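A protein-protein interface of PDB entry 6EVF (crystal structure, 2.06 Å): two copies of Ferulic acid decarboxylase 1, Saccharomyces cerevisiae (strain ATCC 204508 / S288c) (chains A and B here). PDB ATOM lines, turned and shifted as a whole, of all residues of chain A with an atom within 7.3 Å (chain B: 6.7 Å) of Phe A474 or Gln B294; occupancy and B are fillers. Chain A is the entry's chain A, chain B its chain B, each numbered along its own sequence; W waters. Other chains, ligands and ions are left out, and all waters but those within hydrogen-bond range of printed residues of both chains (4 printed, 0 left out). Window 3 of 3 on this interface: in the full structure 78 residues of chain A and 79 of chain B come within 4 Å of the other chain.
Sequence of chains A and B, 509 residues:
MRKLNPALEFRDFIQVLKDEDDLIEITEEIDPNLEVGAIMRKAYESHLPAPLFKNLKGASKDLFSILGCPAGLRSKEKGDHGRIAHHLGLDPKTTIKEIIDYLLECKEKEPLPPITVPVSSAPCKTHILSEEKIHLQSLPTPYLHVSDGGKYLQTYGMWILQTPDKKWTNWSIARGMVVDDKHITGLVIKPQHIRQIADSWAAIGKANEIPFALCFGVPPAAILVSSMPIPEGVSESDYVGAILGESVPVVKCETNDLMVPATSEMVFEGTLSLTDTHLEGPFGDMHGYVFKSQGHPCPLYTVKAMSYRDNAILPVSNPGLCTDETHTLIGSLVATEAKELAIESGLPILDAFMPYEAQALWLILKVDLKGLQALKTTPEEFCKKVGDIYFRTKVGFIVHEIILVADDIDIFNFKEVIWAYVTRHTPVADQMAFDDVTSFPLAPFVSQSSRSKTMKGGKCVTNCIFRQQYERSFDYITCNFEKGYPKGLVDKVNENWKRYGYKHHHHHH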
ATOM      1  N   LEU A 369      -2.196  11.710  19.105  1.00  0.00           N
ATOM      2  CA  LEU A 369      -2.000  12.550  17.941  1.00  0.00           C
ATOM      3  C   LEU A 369      -2.121  14.056  18.269  1.00  0.00           C
ATOM      4  O   LEU A 369      -1.378  14.863  17.732  1.00  0.00           O
ATOM      5  CB  LEU A 369      -2.922  12.165  16.785  1.00  0.00           C
ATOM      6  CG  LEU A 369      -2.637  10.883  16.027  1.00  0.00           C
ATOM      7  CD1 LEU A 369      -3.612  10.799  14.836  1.00  0.00           C
ATOM      8  CD2 LEU A 369      -1.154  10.790  15.639  1.00  0.00           C
ATOM      9  N   GLN A 373       0.599  16.808  17.646  1.00  0.00           N
ATOM     10  CA  GLN A 373       0.285  17.998  16.881  1.00  0.00           C
ATOM     11  C   GLN A 373       0.762  19.311  17.625  1.00  0.00           C
ATOM     12  O   GLN A 373       1.235  20.274  16.996  1.00  0.00           O
ATOM     13  CB  GLN A 373      -1.199  18.015  16.505  1.00  0.00           C
ATOM     14  CG  GLN A 373      -1.530  17.025  15.375  1.00  0.00           C
ATOM     15  CD  GLN A 373      -2.982  16.554  15.351  1.00  0.00           C
ATOM     16  OE1 GLN A 373      -3.886  17.195  15.938  1.00  0.00           O
ATOM     17  NE2 GLN A 373      -3.225  15.397  14.666  1.00  0.00           N
ATOM     18  N   ASP A 408      -5.238   5.385  16.675  1.00  0.00           N
ATOM     19  CA  ASP A 408      -6.291   4.471  16.233  1.00  0.00           C
ATOM     20  C   ASP A 408      -5.870   2.975  16.210  1.00  0.00           C
ATOM     21  O   ASP A 408      -6.683   2.135  15.866  1.00  0.00           O
ATOM     22  CB  ASP A 408      -6.844   4.908  14.870  1.00  0.00           C
ATOM     23  CG  ASP A 408      -5.807   4.790  13.710  1.00  0.00           C
ATOM     24  OD1 ASP A 408      -4.582   4.910  13.964  1.00  0.00           O
ATOM     25  OD2 ASP A 408      -6.250   4.585  12.545  1.00  0.00           O
ATOM     26  N   PHE A 466       0.960   8.881   9.496  1.00  0.00           N
ATOM     27  CA  PHE A 466       0.830   9.547   8.199  1.00  0.00           C
ATOM     28  C   PHE A 466       1.224  11.020   8.419  1.00  0.00           C
ATOM     29  O   PHE A 466       0.961  11.581   9.480  1.00  0.00           O
ATOM     30  CB  PHE A 466      -0.645   9.543   7.669  1.00  0.00           C
ATOM     31  CG  PHE A 466      -1.165   8.204   7.231  1.00  0.00           C
ATOM     32  CD1 PHE A 466      -0.618   7.548   6.152  1.00  0.00           C
ATOM     33  CD2 PHE A 466      -2.237   7.625   7.878  1.00  0.00           C
ATOM     34  CE1 PHE A 466      -1.110   6.312   5.732  1.00  0.00           C
ATOM     35  CE2 PHE A 466      -2.720   6.389   7.477  1.00  0.00           C
ATOM     36  CZ  PHE A 466      -2.179   5.746   6.387  1.00  0.00           C
ATOM     37  N   ARG A 467       1.756  11.654   7.382  1.00  0.00           N
ATOM     38  CA  ARG A 467       2.305  12.993   7.507  1.00  0.00           C
ATOM     39  C   ARG A 467       1.247  13.991   8.032  1.00  0.00           C
ATOM     40  O   ARG A 467       1.526  14.791   8.927  1.00  0.00           O
ATOM     41  CB  ARG A 467       2.909  13.431   6.177  1.00  0.00           C
ATOM     42  CG  ARG A 467       3.669  14.729   6.223  1.00  0.00           C
ATOM     43  CD  ARG A 467       4.908  14.681   7.107  1.00  0.00           C
ATOM     44  NE  ARG A 467       5.636  15.971   7.210  1.00  0.00           N
ATOM     45  CZ  ARG A 467       5.259  17.030   7.952  1.00  0.00           C
ATOM     46  NH1 ARG A 467       6.026  18.119   7.975  1.00  0.00           N
ATOM     47  NH2 ARG A 467       4.123  17.027   8.666  1.00  0.00           N
ATOM     48  N   GLN A 468       0.019  13.879   7.552  1.00  0.00           N
ATOM     49  CA  GLN A 468      -1.026  14.768   7.986  1.00  0.00           C
ATOM     50  C   GLN A 468      -1.372  14.604   9.490  1.00  0.00           C
ATOM     51  O   GLN A 468      -1.902  15.526  10.076  1.00  0.00           O
ATOM     52  CB  GLN A 468      -2.273  14.563   7.083  1.00  0.00           C
ATOM     53  CG  GLN A 468      -3.544  15.344   7.500  1.00  0.00           C
ATOM     54  CD  GLN A 468      -4.706  15.129   6.566  1.00  0.00           C
ATOM     55  OE1 GLN A 468      -4.531  14.782   5.359  1.00  0.00           O
ATOM     56  NE2 GLN A 468      -5.909  15.311   7.111  1.00  0.00           N
ATOM     57  N   GLN A 469      -1.139  13.420  10.071  1.00  0.00           N
ATOM     58  CA  GLN A 469      -1.380  13.178  11.514  1.00  0.00           C
ATOM     59  C   GLN A 469      -0.363  13.956  12.399  1.00  0.00           C
ATOM     60  O   GLN A 469      -0.635  14.107  13.601  1.00  0.00           O
ATOM     61  CB  GLN A 469      -1.404  11.678  11.849  1.00  0.00           C
ATOM     62  CG  GLN A 469      -2.511  10.883  11.145  1.00  0.00           C
ATOM     63  CD  GLN A 469      -2.399   9.370  11.329  1.00  0.00           C
ATOM     64  OE1 GLN A 469      -1.295   8.793  11.265  1.00  0.00           O
ATOM     65  NE2 GLN A 469      -3.565   8.712  11.531  1.00  0.00           N
ATOM     66  N   ARG A 472      -2.843  17.751  11.816  1.00  0.00           N
ATOM     67  CA  ARG A 472      -4.286  17.948  12.072  1.00  0.00           C
ATOM     68  C   ARG A 472      -5.037  16.628  12.061  1.00  0.00           C
ATOM     69  O   ARG A 472      -4.459  15.591  11.740  1.00  0.00           O
ATOM     70  CB  ARG A 472      -4.868  18.908  11.004  1.00  0.00           C
ATOM     71  CG  ARG A 472      -4.678  18.440   9.576  1.00  0.00           C
ATOM     72  CD  ARG A 472      -5.045  19.517   8.597  1.00  0.00           C
ATOM     73  NE  ARG A 472      -4.730  19.134   7.219  1.00  0.00           N
ATOM     74  CZ  ARG A 472      -5.599  18.760   6.264  1.00  0.00           C
ATOM     75  NH1 ARG A 472      -6.923  18.699   6.477  1.00  0.00           N
ATOM     76  NH2 ARG A 472      -5.136  18.449   5.044  1.00  0.00           N
ATOM     77  N   SER A 473      -6.329  16.705  12.363  1.00  0.00           N
ATOM     78  CA  SER A 473      -7.266  15.592  12.205  1.00  0.00           C
ATOM     79  C   SER A 473      -7.181  14.996  10.805  1.00  0.00           C
ATOM     80  O   SER A 473      -6.970  15.710   9.809  1.00  0.00           O
ATOM     81  CB  SER A 473      -8.721  16.045  12.433  1.00  0.00           C
ATOM     82  OG  SER A 473      -8.938  16.521  13.746  1.00  0.00           O
ATOM     83  N   PHE A 474      -7.356  13.687  10.739  1.00  0.00           N
ATOM     84  CA  PHE A 474      -7.302  12.989   9.487  1.00  0.00           C
ATOM     85  C   PHE A 474      -8.252  11.801   9.621  1.00  0.00           C
ATOM     86  O   PHE A 474      -7.902  10.762  10.211  1.00  0.00           O
ATOM     87  CB  PHE A 474      -5.864  12.629   9.163  1.00  0.00           C
ATOM     88  CG  PHE A 474      -5.692  11.854   7.850  1.00  0.00           C
ATOM     89  CD1 PHE A 474      -6.599  11.994   6.778  1.00  0.00           C
ATOM     90  CD2 PHE A 474      -4.603  11.006   7.680  1.00  0.00           C
ATOM     91  CE1 PHE A 474      -6.402  11.275   5.584  1.00  0.00           C
ATOM     92  CE2 PHE A 474      -4.425  10.279   6.504  1.00  0.00           C
ATOM     93  CZ  PHE A 474      -5.330  10.406   5.462  1.00  0.00           C
ATOM     94  N   ASP A 475      -9.482  11.973   9.131  1.00  0.00           N
ATOM     95  CA  ASP A 475     -10.550  10.968   9.339  1.00  0.00           C
ATOM     96  C   ASP A 475     -10.658  10.089   8.112  1.00  0.00           C
ATOM     97  O   ASP A 475     -10.943  10.577   7.028  1.00  0.00           O
ATOM     98  CB  ASP A 475     -11.898  11.611   9.649  1.00  0.00           C
ATOM     99  CG  ASP A 475     -11.933  12.225  11.061  1.00  0.00           C
ATOM    100  OD1 ASP A 475     -11.229  11.782  12.008  1.00  0.00           O
ATOM    101  OD2 ASP A 475     -12.687  13.196  11.226  1.00  0.00           O
ATOM    102  N   TYR A 476     -10.346   8.814   8.300  1.00  0.00           N
ATOM    103  CA  TYR A 476     -10.450   7.833   7.246  1.00  0.00           C
ATOM    104  C   TYR A 476     -11.198   6.668   7.838  1.00  0.00           C
ATOM    105  O   TYR A 476     -11.273   6.465   9.072  1.00  0.00           O
ATOM    106  CB  TYR A 476      -9.071   7.411   6.737  1.00  0.00           C
ATOM    107  CG  TYR A 476      -8.049   7.099   7.813  1.00  0.00           C
ATOM    108  CD1 TYR A 476      -8.047   5.901   8.478  1.00  0.00           C
ATOM    109  CD2 TYR A 476      -7.110   8.038   8.192  1.00  0.00           C
ATOM    110  CE1 TYR A 476      -7.139   5.627   9.522  1.00  0.00           C
ATOM    111  CE2 TYR A 476      -6.198   7.786   9.198  1.00  0.00           C
ATOM    112  CZ  TYR A 476      -6.220   6.562   9.857  1.00  0.00           C
ATOM    113  OH  TYR A 476      -5.310   6.306  10.849  1.00  0.00           O
ATOM    114  N   ILE A 477     -11.748   5.885   6.947  1.00  0.00           N
ATOM    115  CA  ILE A 477     -12.460   4.689   7.314  1.00  0.00           C
ATOM    116  C   ILE A 477     -11.510   3.534   7.318  1.00  0.00           C
ATOM    117  O   ILE A 477     -10.811   3.290   6.339  1.00  0.00           O
ATOM    118  CB  ILE A 477     -13.601   4.417   6.319  1.00  0.00           C
ATOM    119  CG1 ILE A 477     -14.554   5.617   6.271  1.00  0.00           C
ATOM    120  CG2 ILE A 477     -14.362   3.156   6.703  1.00  0.00           C
ATOM    121  CD1 ILE A 477     -15.160   6.022   7.612  1.00  0.00           C
ATOM    122  N   ARG B 175     -12.073  -1.874 -10.781  1.00  0.00           N
ATOM    123  CA  ARG B 175     -13.277  -1.365 -10.134  1.00  0.00           C
ATOM    124  C   ARG B 175     -14.061  -0.408 -10.972  1.00  0.00           C
ATOM    125  O   ARG B 175     -13.469   0.368 -11.711  1.00  0.00           O
ATOM    126  CB  ARG B 175     -12.980  -0.675  -8.811  1.00  0.00           C
ATOM    127  CG  ARG B 175     -12.314   0.664  -8.933  1.00  0.00           C
ATOM    128  CD  ARG B 175     -11.644   0.986  -7.624  1.00  0.00           C
ATOM    129  NE  ARG B 175     -11.471   2.434  -7.462  1.00  0.00           N
ATOM    130  CZ  ARG B 175     -10.551   3.026  -6.695  1.00  0.00           C
ATOM    131  NH1 ARG B 175      -9.720   2.317  -5.934  1.00  0.00           N
ATOM    132  NH2 ARG B 175     -10.508   4.369  -6.661  1.00  0.00           N
ATOM    133  N   LEU B 279     -15.523  12.133 -11.656  1.00  0.00           N
ATOM    134  CA  LEU B 279     -14.950  11.940 -10.348  1.00  0.00           C
ATOM    135  C   LEU B 279     -15.276  10.495  -9.910  1.00  0.00           C
ATOM    136  O   LEU B 279     -16.446  10.125  -9.788  1.00  0.00           O
ATOM    137  CB  LEU B 279     -15.514  12.982  -9.367  1.00  0.00           C
ATOM    138  CG  LEU B 279     -15.036  12.878  -7.898  1.00  0.00           C
ATOM    139  CD1 LEU B 279     -13.555  13.289  -7.817  1.00  0.00           C
ATOM    140  CD2 LEU B 279     -15.928  13.709  -6.923  1.00  0.00           C
ATOM    141  N   GLU B 280     -14.238   9.691  -9.695  1.00  0.00           N
ATOM    142  CA  GLU B 280     -14.381   8.293  -9.347  1.00  0.00           C
ATOM    143  C   GLU B 280     -13.742   8.102  -7.987  1.00  0.00           C
ATOM    144  O   GLU B 280     -12.693   8.647  -7.716  1.00  0.00           O
ATOM    145  CB  GLU B 280     -13.640   7.443 -10.388  1.00  0.00           C
ATOM    146  CG  GLU B 280     -13.728   5.939 -10.258  1.00  0.00           C
ATOM    147  CD  GLU B 280     -12.840   5.310  -9.162  1.00  0.00           C
ATOM    148  OE1 GLU B 280     -11.747   5.848  -8.845  1.00  0.00           O
ATOM    149  OE2 GLU B 280     -13.228   4.238  -8.616  1.00  0.00           O
ATOM    150  N   GLY B 281     -14.339   7.256  -7.157  1.00  0.00           N
ATOM    151  CA  GLY B 281     -13.827   7.018  -5.851  1.00  0.00           C
ATOM    152  C   GLY B 281     -14.176   8.111  -4.826  1.00  0.00           C
ATOM    153  O   GLY B 281     -14.896   9.074  -5.119  1.00  0.00           O
ATOM    154  N   PRO B 282     -13.658   7.971  -3.609  1.00  0.00           N
ATOM    155  CA  PRO B 282     -12.752   6.921  -3.214  1.00  0.00           C
ATOM    156  C   PRO B 282     -13.464   5.565  -3.050  1.00  0.00           C
ATOM    157  O   PRO B 282     -14.708   5.464  -3.143  1.00  0.00           O
ATOM    158  CB  PRO B 282     -12.241   7.432  -1.860  1.00  0.00           C
ATOM    159  CG  PRO B 282     -13.444   8.149  -1.321  1.00  0.00           C
ATOM    160  CD  PRO B 282     -14.000   8.870  -2.482  1.00  0.00           C
ATOM    161  N   PHE B 283     -12.662   4.526  -2.896  1.00  0.00           N
ATOM    162  CA  PHE B 283     -13.167   3.172  -2.669  1.00  0.00           C
ATOM    163  C   PHE B 283     -12.281   2.489  -1.619  1.00  0.00           C
ATOM    164  O   PHE B 283     -11.063   2.595  -1.672  1.00  0.00           O
ATOM    165  CB  PHE B 283     -13.145   2.388  -3.983  1.00  0.00           C
ATOM    166  CG  PHE B 283     -13.709   0.962  -3.895  1.00  0.00           C
ATOM    167  CD1 PHE B 283     -15.021   0.743  -3.518  1.00  0.00           C
ATOM    168  CD2 PHE B 283     -12.954  -0.135  -4.288  1.00  0.00           C
ATOM    169  CE1 PHE B 283     -15.561  -0.537  -3.534  1.00  0.00           C
ATOM    170  CE2 PHE B 283     -13.485  -1.430  -4.272  1.00  0.00           C
ATOM    171  CZ  PHE B 283     -14.786  -1.624  -3.909  1.00  0.00           C
ATOM    172  N   PHE B 291     -10.210   6.687   2.022  1.00  0.00           N
ATOM    173  CA  PHE B 291      -9.689   8.038   2.223  1.00  0.00           C
ATOM    174  C   PHE B 291     -10.748   9.042   1.736  1.00  0.00           C
ATOM    175  O   PHE B 291     -10.952   9.214   0.542  1.00  0.00           O
ATOM    176  CB  PHE B 291      -8.314   8.187   1.551  1.00  0.00           C
ATOM    177  CG  PHE B 291      -7.190   7.425   2.271  1.00  0.00           C
ATOM    178  CD1 PHE B 291      -6.884   7.702   3.605  1.00  0.00           C
ATOM    179  CD2 PHE B 291      -6.434   6.471   1.617  1.00  0.00           C
ATOM    180  CE1 PHE B 291      -5.898   7.011   4.287  1.00  0.00           C
ATOM    181  CE2 PHE B 291      -5.426   5.793   2.293  1.00  0.00           C
ATOM    182  CZ  PHE B 291      -5.172   6.044   3.623  1.00  0.00           C
ATOM    183  N   LYS B 292     -11.441   9.638   2.695  1.00  0.00           N
ATOM    184  CA  LYS B 292     -12.635  10.422   2.436  1.00  0.00           C
ATOM    185  C   LYS B 292     -12.352  11.519   1.516  1.00  0.00           C
ATOM    186  O   LYS B 292     -11.284  12.164   1.624  1.00  0.00           O
ATOM    187  CB  LYS B 292     -13.231  11.019   3.708  1.00  0.00           C
ATOM    188  CG  LYS B 292     -13.814   9.979   4.670  1.00  0.00           C
ATOM    189  CD  LYS B 292     -14.330  10.609   5.973  1.00  0.00           C
ATOM    190  CE  LYS B 292     -14.667   9.508   6.971  1.00  0.00           C
ATOM    191  NZ  LYS B 292     -15.490  10.069   8.058  1.00  0.00           N
ATOM    192  N   SER B 293     -13.291  11.682   0.556  1.00  0.00           N
ATOM    193  CA  SER B 293     -13.251  12.716  -0.489  1.00  0.00           C
ATOM    194  C   SER B 293     -11.956  12.742  -1.266  1.00  0.00           C
ATOM    195  O   SER B 293     -11.613  13.807  -1.775  1.00  0.00           O
ATOM    196  CB  SER B 293     -13.456  14.144   0.112  1.00  0.00           C
ATOM    197  OG  SER B 293     -14.618  14.270   0.854  1.00  0.00           O
ATOM    198  N   GLN B 294     -11.264  11.603  -1.381  1.00  0.00           N
ATOM    199  CA  GLN B 294     -10.042  11.519  -2.164  1.00  0.00           C
ATOM    200  C   GLN B 294     -10.287  10.773  -3.482  1.00  0.00           C
ATOM    201  O   GLN B 294      -9.527   9.843  -3.871  1.00  0.00           O
ATOM    202  CB  GLN B 294      -8.902  10.882  -1.364  1.00  0.00           C
ATOM    203  CG  GLN B 294      -8.560  11.710  -0.123  1.00  0.00           C
ATOM    204  CD  GLN B 294      -7.170  11.444   0.377  1.00  0.00           C
ATOM    205  OE1 GLN B 294      -6.310  11.027  -0.406  1.00  0.00           O
ATOM    206  NE2 GLN B 294      -6.949  11.603   1.708  1.00  0.00           N
ATOM    207  N   GLY B 295     -11.360  11.190  -4.148  1.00  0.00           N
ATOM    208  CA  GLY B 295     -11.632  10.786  -5.540  1.00  0.00           C
ATOM    209  C   GLY B 295     -10.789  11.557  -6.537  1.00  0.00           C
ATOM    210  O   GLY B 295     -10.187  12.590  -6.189  1.00  0.00           O
ATOM    211  N   HIS B 296     -10.753  11.034  -7.774  1.00  0.00           N
ATOM    212  CA  HIS B 296      -9.902  11.536  -8.862  1.00  0.00           C
ATOM    213  C   HIS B 296     -10.635  11.220 -10.176  1.00  0.00           C
ATOM    214  O   HIS B 296     -11.478  10.301 -10.227  1.00  0.00           O
ATOM    215  CB  HIS B 296      -8.519  10.855  -8.890  1.00  0.00           C
ATOM    216  CG  HIS B 296      -7.754  10.910  -7.595  1.00  0.00           C
ATOM    217  ND1 HIS B 296      -7.346  12.093  -7.006  1.00  0.00           N
ATOM    218  CD2 HIS B 296      -7.264   9.913  -6.807  1.00  0.00           C
ATOM    219  CE1 HIS B 296      -6.682  11.823  -5.891  1.00  0.00           C
ATOM    220  NE2 HIS B 296      -6.617  10.510  -5.748  1.00  0.00           N
ATOM    221  N   SER B 447       0.009   7.228  -1.399  1.00  0.00           N
ATOM    222  CA  SER B 447      -1.076   8.192  -1.698  1.00  0.00           C
ATOM    223  C   SER B 447      -1.165   9.348  -0.698  1.00  0.00           C
ATOM    224  O   SER B 447      -1.528  10.426  -1.066  1.00  0.00           O
ATOM    225  CB  SER B 447      -2.439   7.479  -1.834  1.00  0.00           C
ATOM    226  OG  SER B 447      -2.912   6.887  -0.625  1.00  0.00           O
ATOM    227  N   GLN B 448      -0.731   9.147   0.551  1.00  0.00           N
ATOM    228  CA  GLN B 448      -0.936  10.133   1.587  1.00  0.00           C
ATOM    229  C   GLN B 448       0.399  10.819   1.943  1.00  0.00           C
ATOM    230  O   GLN B 448       0.611  11.239   3.065  1.00  0.00           O
ATOM    231  CB  GLN B 448      -1.517   9.428   2.807  1.00  0.00           C
ATOM    232  CG  GLN B 448      -2.853   8.740   2.606  1.00  0.00           C
ATOM    233  CD  GLN B 448      -3.838   9.608   1.857  1.00  0.00           C
ATOM    234  OE1 GLN B 448      -4.210   9.283   0.751  1.00  0.00           O
ATOM    235  NE2 GLN B 448      -4.214  10.717   2.431  1.00  0.00           N
HETATM  236  O   HOH W   1       2.189   9.992   5.013  1.00  0.00           O
HETATM  237  O   HOH W   2      -3.164  12.740   4.025  1.00  0.00           O
HETATM  238  O   HOH W   3      -9.683  10.304   4.910  1.00  0.00           O
HETATM  239  O   HOH W   4      -0.808  12.217   5.270  1.00  0.00           O
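Phe A474 touches just these residues of chain B: Phe B291 (3.6 Å), Gln B294 (3.9 Å) and Gln B448 (3.2 Å).
Gln B294 touches one residue of chain A.
Of the printed residues of chain B, Tyr A476 touches Phe B291.
Of the printed residues of chain B, Ile A477 touches Lys B292.
Printed residues of chain B within 4 Å of Phe A466: Gln B448.
Printed residues of chain A within 4 Å of Gln B448: Phe A466 and Phe A474.
Of the printed residues of chain A, Phe B291 touches Phe A474 (3.6 Å) and Tyr A476 (3.8 Å).
Gly B281 touches none of the printed residues of chain A.
Phe B283 touches none of the printed residues of chain A.
The nearest residue of chain B that does not touch Phe A474 is Lys B292 (6.0 Å).
No position is printed for both chains.
Of the 7 pairs that touch across the chains among the printed residues, none has its exchanged pair printed and touching as well.
Water W3 bridges the backbone carbonyl oxygen of Asp A475 and the backbone NH of Lys B292.
Water W2 bridges NE2 of Gln B448 (2.8 Å) and OE1 of Gln A468 (2.8 Å).
Water W4 lies within hydrogen-bond range of O of Gln B448 (2.8 Å), N of Gln A468 (2.9 Å) and N of Arg A467 (3.4 Å).
Water W1 lies within hydrogen-bond range of O of Gln B448 and N of Arg A467.
Of the 14 printed residues of chain B, 4 touch a printed residue of chain A.
Hydrophobic or aromatic side chains of chain B within 4 Å of the printed part of chain A: Phe B291.
Printed residues of chain A that touch a printed residue of chain B: Phe A466, Phe A474, Asp A475, Tyr A476 and Ile A477.
Hydrophobic or aromatic side chains of chain A that line the printed part of chain B: Phe A466, Phe A474, Tyr A476 and Ile A477.
Among the printed residues, 7 pairs touch across the chains.
Among the printed residues, no Asp or Glu carboxylate lies within 4 Å of a Lys or Arg side-chain nitrogen of the other chain.
Among the printed residues, pairs that only touch across the chains: Phe A466 with Gln B448, Phe A474 with Phe B291, Phe A474 with Gln B294, Phe A474 with Gln B448, Asp A475 with Lys B292, Tyr A476 with Phe B291 and Ile A477 with Lys B292.
OH of Tyr A476 is in hydrogen-bond range of NE2 of Gln A469, at 3.0 Å.
OH of Tyr A476 lies within hydrogen-bond range of OD2 of Asp A408 (2.6 Å).
The backbone NH (N) of Phe A466 is in hydrogen-bond range of the side-chain amide oxygen (OE1) of Gln A469 (2.9 Å).
The side-chain hydroxyl (OG) of Ser B447 sits at hydrogen-bond distance from the side-chain amide oxygen (OE1) of Gln B448 (3.1 Å).
OE1 of Gln B294 sits close to OE1 of Gln B448.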
